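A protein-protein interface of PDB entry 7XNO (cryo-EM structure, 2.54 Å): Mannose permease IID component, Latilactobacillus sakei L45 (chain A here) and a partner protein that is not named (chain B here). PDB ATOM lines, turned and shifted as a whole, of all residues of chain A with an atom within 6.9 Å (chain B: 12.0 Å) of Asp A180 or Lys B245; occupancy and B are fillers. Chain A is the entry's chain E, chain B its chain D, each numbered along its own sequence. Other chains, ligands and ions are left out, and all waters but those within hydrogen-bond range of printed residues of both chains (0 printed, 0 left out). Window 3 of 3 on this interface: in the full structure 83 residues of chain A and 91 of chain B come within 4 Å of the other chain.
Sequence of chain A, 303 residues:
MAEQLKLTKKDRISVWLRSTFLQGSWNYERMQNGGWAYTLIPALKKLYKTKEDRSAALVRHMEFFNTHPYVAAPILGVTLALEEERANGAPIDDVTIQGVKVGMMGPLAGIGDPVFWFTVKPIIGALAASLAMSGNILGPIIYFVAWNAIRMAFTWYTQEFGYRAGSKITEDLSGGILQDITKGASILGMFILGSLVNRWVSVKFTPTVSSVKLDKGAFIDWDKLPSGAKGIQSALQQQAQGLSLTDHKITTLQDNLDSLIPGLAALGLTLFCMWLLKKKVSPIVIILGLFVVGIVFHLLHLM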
ATOM      1  N   GLY A 176     -22.220  -4.783  27.077  1.00  0.00           N
ATOM      2  CA  GLY A 176     -22.325  -3.709  26.115  1.00  0.00           C
ATOM      3  C   GLY A 176     -23.620  -2.934  26.164  1.00  0.00           C
ATOM      4  O   GLY A 176     -23.764  -1.939  25.447  1.00  0.00           O
ATOM      5  N   ILE A 177     -24.577  -3.367  26.988  1.00  0.00           N
ATOM      6  CA  ILE A 177     -25.831  -2.635  27.129  1.00  0.00           C
ATOM      7  C   ILE A 177     -25.598  -1.280  27.788  1.00  0.00           C
ATOM      8  O   ILE A 177     -26.279  -0.297  27.461  1.00  0.00           O
ATOM      9  CB  ILE A 177     -26.857  -3.487  27.904  1.00  0.00           C
ATOM     10  CG1 ILE A 177     -28.213  -2.780  27.965  1.00  0.00           C
ATOM     11  CG2 ILE A 177     -26.348  -3.829  29.300  1.00  0.00           C
ATOM     12  CD1 ILE A 177     -28.877  -2.618  26.617  1.00  0.00           C
ATOM     13  N   LEU A 178     -24.643  -1.197  28.715  1.00  0.00           N
ATOM     14  CA  LEU A 178     -24.343   0.047  29.408  1.00  0.00           C
ATOM     15  C   LEU A 178     -23.771   1.117  28.489  1.00  0.00           C
ATOM     16  O   LEU A 178     -23.797   2.297  28.853  1.00  0.00           O
ATOM     17  CB  LEU A 178     -23.369  -0.212  30.561  1.00  0.00           C
ATOM     18  CG  LEU A 178     -23.925  -0.955  31.776  1.00  0.00           C
ATOM     19  CD1 LEU A 178     -22.999  -0.791  32.970  1.00  0.00           C
ATOM     20  CD2 LEU A 178     -25.328  -0.474  32.112  1.00  0.00           C
ATOM     21  N   GLN A 179     -23.256   0.742  27.320  1.00  0.00           N
ATOM     22  CA  GLN A 179     -22.821   1.710  26.323  1.00  0.00           C
ATOM     23  C   GLN A 179     -23.984   2.303  25.544  1.00  0.00           C
ATOM     24  O   GLN A 179     -24.036   3.521  25.348  1.00  0.00           O
ATOM     25  CB  GLN A 179     -21.833   1.061  25.347  1.00  0.00           C
ATOM     26  CG  GLN A 179     -20.400   1.034  25.845  1.00  0.00           C
ATOM     27  CD  GLN A 179     -20.208   0.098  27.020  1.00  0.00           C
ATOM     28  OE1 GLN A 179     -20.388  -1.114  26.901  1.00  0.00           O
ATOM     29  NE2 GLN A 179     -19.852   0.659  28.170  1.00  0.00           N
ATOM     30  N   ASP A 180     -24.929   1.466  25.110  1.00  0.00           N
ATOM     31  CA  ASP A 180     -26.113   1.975  24.429  1.00  0.00           C
ATOM     32  C   ASP A 180     -26.961   2.824  25.364  1.00  0.00           C
ATOM     33  O   ASP A 180     -27.489   3.869  24.960  1.00  0.00           O
ATOM     34  CB  ASP A 180     -26.930   0.812  23.868  1.00  0.00           C
ATOM     35  CG  ASP A 180     -26.066  -0.216  23.166  1.00  0.00           C
ATOM     36  OD1 ASP A 180     -25.199   0.184  22.362  1.00  0.00           O
ATOM     37  OD2 ASP A 180     -26.253  -1.425  23.420  1.00  0.00           O
ATOM     38  N   ILE A 181     -27.106   2.389  26.619  1.00  0.00           N
ATOM     39  CA  ILE A 181     -27.862   3.174  27.590  1.00  0.00           C
ATOM     40  C   ILE A 181     -27.195   4.524  27.814  1.00  0.00           C
ATOM     41  O   ILE A 181     -27.864   5.562  27.852  1.00  0.00           O
ATOM     42  CB  ILE A 181     -28.018   2.393  28.908  1.00  0.00           C
ATOM     43  CG1 ILE A 181     -28.915   1.173  28.703  1.00  0.00           C
ATOM     44  CG2 ILE A 181     -28.586   3.288  29.997  1.00  0.00           C
ATOM     45  CD1 ILE A 181     -29.012   0.278  29.917  1.00  0.00           C
ATOM     46  N   THR A 182     -25.868   4.530  27.955  1.00  0.00           N
ATOM     47  CA  THR A 182     -25.147   5.785  28.149  1.00  0.00           C
ATOM     48  C   THR A 182     -25.298   6.702  26.942  1.00  0.00           C
ATOM     49  O   THR A 182     -25.488   7.912  27.094  1.00  0.00           O
ATOM     50  CB  THR A 182     -23.671   5.502  28.435  1.00  0.00           C
ATOM     51  OG1 THR A 182     -23.539   4.936  29.743  1.00  0.00           O
ATOM     52  CG2 THR A 182     -22.850   6.778  28.364  1.00  0.00           C
ATOM     53  N   LYS A 183     -25.230   6.143  25.731  1.00  0.00           N
ATOM     54  CA  LYS A 183     -25.378   6.948  24.521  1.00  0.00           C
ATOM     55  C   LYS A 183     -26.765   7.578  24.434  1.00  0.00           C
ATOM     56  O   LYS A 183     -26.905   8.783  24.175  1.00  0.00           O
ATOM     57  CB  LYS A 183     -25.105   6.080  23.295  1.00  0.00           C
ATOM     58  CG  LYS A 183     -25.086   6.840  21.989  1.00  0.00           C
ATOM     59  CD  LYS A 183     -23.688   7.301  21.648  1.00  0.00           C
ATOM     60  CE  LYS A 183     -23.673   8.025  20.320  1.00  0.00           C
ATOM     61  NZ  LYS A 183     -24.186   9.415  20.450  1.00  0.00           N
ATOM     62  N   GLY A 184     -27.809   6.770  24.635  1.00  0.00           N
ATOM     63  CA  GLY A 184     -29.160   7.303  24.576  1.00  0.00           C
ATOM     64  C   GLY A 184     -29.424   8.324  25.664  1.00  0.00           C
ATOM     65  O   GLY A 184     -30.083   9.345  25.430  1.00  0.00           O
ATOM     66  N   ALA A 185     -28.910   8.068  26.869  1.00  0.00           N
ATOM     67  CA  ALA A 185     -29.050   9.026  27.955  1.00  0.00           C
ATOM     68  C   ALA A 185     -28.318  10.320  27.637  1.00  0.00           C
ATOM     69  O   ALA A 185     -28.800  11.404  27.968  1.00  0.00           O
ATOM     70  CB  ALA A 185     -28.532   8.421  29.257  1.00  0.00           C
ATOM     71  N   SER A 186     -27.158  10.229  26.987  1.00  0.00           N
ATOM     72  CA  SER A 186     -26.432  11.433  26.602  1.00  0.00           C
ATOM     73  C   SER A 186     -27.224  12.254  25.594  1.00  0.00           C
ATOM     74  O   SER A 186     -27.310  13.481  25.713  1.00  0.00           O
ATOM     75  CB  SER A 186     -25.063  11.062  26.037  1.00  0.00           C
ATOM     76  OG  SER A 186     -24.410  12.196  25.496  1.00  0.00           O
ATOM     77  N   MET B 203     -21.291  15.726  29.987  1.00  0.00           N
ATOM     78  CA  MET B 203     -21.920  14.875  28.983  1.00  0.00           C
ATOM     79  C   MET B 203     -21.976  15.499  27.589  1.00  0.00           C
ATOM     80  O   MET B 203     -22.833  15.118  26.787  1.00  0.00           O
ATOM     81  CB  MET B 203     -23.321  14.490  29.456  1.00  0.00           C
ATOM     82  CG  MET B 203     -24.273  15.658  29.573  1.00  0.00           C
ATOM     83  SD  MET B 203     -25.899  15.138  30.121  1.00  0.00           S
ATOM     84  CE  MET B 203     -26.449  14.322  28.643  1.00  0.00           C
ATOM     85  N   GLU B 207     -20.712  15.021  18.910  1.00  0.00           N
ATOM     86  CA  GLU B 207     -21.731  14.208  18.262  1.00  0.00           C
ATOM     87  C   GLU B 207     -23.121  14.420  18.851  1.00  0.00           C
ATOM     88  O   GLU B 207     -24.115  14.059  18.209  1.00  0.00           O
ATOM     89  CB  GLU B 207     -21.326  12.730  18.353  1.00  0.00           C
ATOM     90  CG  GLU B 207     -22.263  11.740  17.689  1.00  0.00           C
ATOM     91  CD  GLU B 207     -22.048  10.330  18.190  1.00  0.00           C
ATOM     92  OE1 GLU B 207     -21.647  10.177  19.363  1.00  0.00           O
ATOM     93  OE2 GLU B 207     -22.279   9.377  17.418  1.00  0.00           O
ATOM     94  N   VAL B 208     -23.222  15.028  20.033  1.00  0.00           N
ATOM     95  CA  VAL B 208     -24.511  15.266  20.677  1.00  0.00           C
ATOM     96  C   VAL B 208     -24.863  16.742  20.782  1.00  0.00           C
ATOM     97  O   VAL B 208     -25.983  17.064  21.212  1.00  0.00           O
ATOM     98  CB  VAL B 208     -24.577  14.613  22.074  1.00  0.00           C
ATOM     99  CG1 VAL B 208     -24.658  13.099  21.949  1.00  0.00           C
ATOM    100  CG2 VAL B 208     -23.381  15.023  22.909  1.00  0.00           C
ATOM    101  N   PHE B 211     -28.211  17.811  19.093  1.00  0.00           N
ATOM    102  CA  PHE B 211     -29.415  17.564  19.880  1.00  0.00           C
ATOM    103  C   PHE B 211     -29.637  18.670  20.904  1.00  0.00           C
ATOM    104  O   PHE B 211     -30.779  19.078  21.149  1.00  0.00           O
ATOM    105  CB  PHE B 211     -29.325  16.200  20.560  1.00  0.00           C
ATOM    106  CG  PHE B 211     -29.188  15.059  19.596  1.00  0.00           C
ATOM    107  CD1 PHE B 211     -30.295  14.552  18.940  1.00  0.00           C
ATOM    108  CD2 PHE B 211     -27.948  14.499  19.339  1.00  0.00           C
ATOM    109  CE1 PHE B 211     -30.171  13.504  18.049  1.00  0.00           C
ATOM    110  CE2 PHE B 211     -27.816  13.452  18.451  1.00  0.00           C
ATOM    111  CZ  PHE B 211     -28.929  12.954  17.805  1.00  0.00           C
ATOM    112  N   GLY B 233     -37.035  14.082  22.737  1.00  0.00           N
ATOM    113  CA  GLY B 233     -35.644  13.705  22.933  1.00  0.00           C
ATOM    114  C   GLY B 233     -35.444  12.203  22.992  1.00  0.00           C
ATOM    115  O   GLY B 233     -34.490  11.671  22.419  1.00  0.00           O
ATOM    116  N   ILE B 234     -36.343  11.497  23.683  1.00  0.00           N
ATOM    117  CA  ILE B 234     -36.248  10.042  23.766  1.00  0.00           C
ATOM    118  C   ILE B 234     -36.428   9.416  22.389  1.00  0.00           C
ATOM    119  O   ILE B 234     -35.699   8.491  22.010  1.00  0.00           O
ATOM    120  CB  ILE B 234     -37.271   9.494  24.777  1.00  0.00           C
ATOM    121  CG1 ILE B 234     -36.893   9.910  26.198  1.00  0.00           C
ATOM    122  CG2 ILE B 234     -37.367   7.980  24.681  1.00  0.00           C
ATOM    123  CD1 ILE B 234     -37.977   9.649  27.215  1.00  0.00           C
ATOM    124  N   SER B 235     -37.403   9.907  21.619  1.00  0.00           N
ATOM    125  CA  SER B 235     -37.621   9.384  20.276  1.00  0.00           C
ATOM    126  C   SER B 235     -36.418   9.644  19.377  1.00  0.00           C
ATOM    127  O   SER B 235     -36.024   8.776  18.590  1.00  0.00           O
ATOM    128  CB  SER B 235     -38.883   9.998  19.675  1.00  0.00           C
ATOM    129  OG  SER B 235     -39.978   9.875  20.564  1.00  0.00           O
ATOM    130  N   LEU B 236     -35.826  10.836  19.476  1.00  0.00           N
ATOM    131  CA  LEU B 236     -34.648  11.145  18.675  1.00  0.00           C
ATOM    132  C   LEU B 236     -33.477  10.249  19.054  1.00  0.00           C
ATOM    133  O   LEU B 236     -32.743   9.774  18.180  1.00  0.00           O
ATOM    134  CB  LEU B 236     -34.273  12.618  18.836  1.00  0.00           C
ATOM    135  CG  LEU B 236     -35.161  13.623  18.105  1.00  0.00           C
ATOM    136  CD1 LEU B 236     -34.564  15.018  18.178  1.00  0.00           C
ATOM    137  CD2 LEU B 236     -35.370  13.199  16.661  1.00  0.00           C
ATOM    138  N   ALA B 237     -33.285  10.009  20.353  1.00  0.00           N
ATOM    139  CA  ALA B 237     -32.227   9.103  20.787  1.00  0.00           C
ATOM    140  C   ALA B 237     -32.457   7.693  20.258  1.00  0.00           C
ATOM    141  O   ALA B 237     -31.518   7.033  19.800  1.00  0.00           O
ATOM    142  CB  ALA B 237     -32.134   9.095  22.312  1.00  0.00           C
ATOM    143  N   LEU B 238     -33.702   7.215  20.316  1.00  0.00           N
ATOM    144  CA  LEU B 238     -34.008   5.878  19.816  1.00  0.00           C
ATOM    145  C   LEU B 238     -33.754   5.775  18.316  1.00  0.00           C
ATOM    146  O   LEU B 238     -33.185   4.786  17.843  1.00  0.00           O
ATOM    147  CB  LEU B 238     -35.455   5.515  20.140  1.00  0.00           C
ATOM    148  CG  LEU B 238     -35.766   5.177  21.599  1.00  0.00           C
ATOM    149  CD1 LEU B 238     -37.267   5.129  21.828  1.00  0.00           C
ATOM    150  CD2 LEU B 238     -35.119   3.862  21.998  1.00  0.00           C
ATOM    151  N   ILE B 239     -34.163   6.793  17.557  1.00  0.00           N
ATOM    152  CA  ILE B 239     -33.955   6.777  16.111  1.00  0.00           C
ATOM    153  C   ILE B 239     -32.467   6.820  15.784  1.00  0.00           C
ATOM    154  O   ILE B 239     -31.991   6.107  14.891  1.00  0.00           O
ATOM    155  CB  ILE B 239     -34.720   7.939  15.452  1.00  0.00           C
ATOM    156  CG1 ILE B 239     -36.224   7.656  15.454  1.00  0.00           C
ATOM    157  CG2 ILE B 239     -34.230   8.178  14.034  1.00  0.00           C
ATOM    158  CD1 ILE B 239     -37.078   8.902  15.393  1.00  0.00           C
ATOM    159  N   TYR B 240     -31.710   7.656  16.500  1.00  0.00           N
ATOM    160  CA  TYR B 240     -30.273   7.740  16.272  1.00  0.00           C
ATOM    161  C   TYR B 240     -29.588   6.416  16.581  1.00  0.00           C
ATOM    162  O   TYR B 240     -28.725   5.964  15.822  1.00  0.00           O
ATOM    163  CB  TYR B 240     -29.679   8.864  17.119  1.00  0.00           C
ATOM    164  CG  TYR B 240     -28.291   9.288  16.707  1.00  0.00           C
ATOM    165  CD1 TYR B 240     -28.102  10.231  15.707  1.00  0.00           C
ATOM    166  CD2 TYR B 240     -27.168   8.750  17.319  1.00  0.00           C
ATOM    167  CE1 TYR B 240     -26.836  10.624  15.328  1.00  0.00           C
ATOM    168  CE2 TYR B 240     -25.899   9.137  16.946  1.00  0.00           C
ATOM    169  CZ  TYR B 240     -25.737  10.074  15.950  1.00  0.00           C
ATOM    170  OH  TYR B 240     -24.473  10.464  15.574  1.00  0.00           O
ATOM    171  N   LEU B 241     -29.967   5.772  17.688  1.00  0.00           N
ATOM    172  CA  LEU B 241     -29.390   4.473  18.016  1.00  0.00           C
ATOM    173  C   LEU B 241     -29.741   3.430  16.964  1.00  0.00           C
ATOM    174  O   LEU B 241     -28.888   2.629  16.565  1.00  0.00           O
ATOM    175  CB  LEU B 241     -29.861   4.024  19.398  1.00  0.00           C
ATOM    176  CG  LEU B 241     -29.232   4.746  20.591  1.00  0.00           C
ATOM    177  CD1 LEU B 241     -29.832   4.249  21.894  1.00  0.00           C
ATOM    178  CD2 LEU B 241     -27.725   4.566  20.593  1.00  0.00           C
ATOM    179  N   ALA B 242     -30.992   3.428  16.496  1.00  0.00           N
ATOM    180  CA  ALA B 242     -31.401   2.466  15.478  1.00  0.00           C
ATOM    181  C   ALA B 242     -30.621   2.661  14.185  1.00  0.00           C
ATOM    182  O   ALA B 242     -30.194   1.684  13.559  1.00  0.00           O
ATOM    183  CB  ALA B 242     -32.903   2.579  15.223  1.00  0.00           C
ATOM    184  N   LEU B 243     -30.422   3.908  13.770  1.00  0.00           N
ATOM    185  CA  LEU B 243     -29.674   4.199  12.555  1.00  0.00           C
ATOM    186  C   LEU B 243     -28.168   4.058  12.735  1.00  0.00           C
ATOM    187  O   LEU B 243     -27.443   4.003  11.736  1.00  0.00           O
ATOM    188  CB  LEU B 243     -30.005   5.609  12.058  1.00  0.00           C
ATOM    189  CG  LEU B 243     -31.409   5.793  11.477  1.00  0.00           C
ATOM    190  CD1 LEU B 243     -31.639   7.237  11.067  1.00  0.00           C
ATOM    191  CD2 LEU B 243     -31.628   4.862  10.301  1.00  0.00           C
ATOM    192  N   SER B 244     -27.680   4.003  13.974  1.00  0.00           N
ATOM    193  CA  SER B 244     -26.259   3.824  14.238  1.00  0.00           C
ATOM    194  C   SER B 244     -25.842   2.375  14.420  1.00  0.00           C
ATOM    195  O   SER B 244     -24.708   2.031  14.082  1.00  0.00           O
ATOM    196  CB  SER B 244     -25.848   4.614  15.487  1.00  0.00           C
ATOM    197  OG  SER B 244     -25.621   5.976  15.175  1.00  0.00           O
ATOM    198  N   LYS B 245     -26.719   1.519  14.953  1.00  0.00           N
ATOM    199  CA  LYS B 245     -26.356   0.114  15.123  1.00  0.00           C
ATOM    200  C   LYS B 245     -26.128  -0.572  13.784  1.00  0.00           C
ATOM    201  O   LYS B 245     -25.335  -1.517  13.702  1.00  0.00           O
ATOM    202  CB  LYS B 245     -27.433  -0.626  15.915  1.00  0.00           C
ATOM    203  CG  LYS B 245     -27.658  -0.084  17.312  1.00  0.00           C
ATOM    204  CD  LYS B 245     -26.440  -0.286  18.191  1.00  0.00           C
ATOM    205  CE  LYS B 245     -26.634   0.378  19.541  1.00  0.00           C
ATOM    206  NZ  LYS B 245     -27.704  -0.280  20.336  1.00  0.00           N
ATOM    207  N   GLN B 246     -26.808  -0.120  12.732  1.00  0.00           N
ATOM    208  CA  GLN B 246     -26.637  -0.685  11.393  1.00  0.00           C
ATOM    209  C   GLN B 246     -25.545   0.084  10.644  1.00  0.00           C
ATOM    210  O   GLN B 246     -25.690   0.510   9.496  1.00  0.00           O
ATOM    211  CB  GLN B 246     -27.971  -0.685  10.653  1.00  0.00           C
ATOM    212  CG  GLN B 246     -28.547   0.695  10.365  1.00  0.00           C
ATOM    213  CD  GLN B 246     -29.898   0.628   9.683  1.00  0.00           C
ATOM    214  OE1 GLN B 246     -30.395  -0.453   9.371  1.00  0.00           O
ATOM    215  NE2 GLN B 246     -30.502   1.787   9.456  1.00  0.00           N
ATOM    216  N   GLY B 247     -24.410   0.227  11.321  1.00  0.00           N
ATOM    217  CA  GLY B 247     -23.272   0.932  10.762  1.00  0.00           C
ATOM    218  C   GLY B 247     -22.065   0.931  11.679  1.00  0.00           C
ATOM    219  O   GLY B 247     -22.124   0.417  12.796  1.00  0.00           O
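The side-chain carboxylate (OE1) of Glu B207 is in salt-bridge range of the side-chain amino group (NZ) of Lys A183 (2.9 Å). The side-chain amino group of Lys B245 lies within salt-bridge range of the side-chain carboxylate of Asp A180 (3.3 Å).
O of Tyr B240 is in hydrogen-bond range of OG of Ser B244 (3.2 Å). The side-chain carboxylate of Glu B207 sits at hydrogen-bond distance from the side-chain hydroxyl of Tyr B240 (3.1 Å).
Among the printed residues, merely in contact across the chains: Ser A186 with Met B203, Ser A186 with Val B208, Gly A184 with Ala B237, Lys A183 with Leu B241, Ala A185 with Met B203, Asp A180 with Leu B241 and Lys A183 with Tyr B240.
No residue of chain B comes within 4 Å of Gly A176. Ile A177 touches none of the printed residues of chain B. No residue of chain B comes within 4 Å of Gln A179. Asp A180 touches just these residues of chain B: Leu B241 and Lys B245. No residue of chain B comes within 4 Å of Ile A181. No residue of chain B comes within 4 Å of Thr A182. Of the printed residues of chain B, Lys A183 touches Glu B207 (2.9 Å), Tyr B240 (3.9 Å) and Leu B241 (3.8 Å). Gly A184 touches one residue of chain B. Printed residues of chain A within 4 Å of Glu B207: Lys A183. Of the printed residues of chain A, Ala B237 touches Gly A184 (3.7 Å). Of chain A, only Asp A180 comes within 4 Å of Lys B245. The nearest residue of chain B that does not touch Asp A180 is Ala B237 (7.3 Å). The nearest printed residue of chain B that does not touch Ala A185 is Ala B237 (5.7 Å).
Of the 11 printed residues of chain A, 5 touch a printed residue of chain B. Of the 19 printed residues of chain B, 7 touch a printed residue of chain A. Printed residues of chain B that touch a printed residue of chain A: Met B203, Glu B207, Val B208, Ala B237, Tyr B240, Leu B241 and Lys B245. Among the printed residues, Asp or Glu carboxylates within 4 Å of a Lys or Arg side-chain nitrogen of the other chain: Asp A180 with Lys B245 (3.3 Å) and Lys A183 with Glu B207 (2.9 Å).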
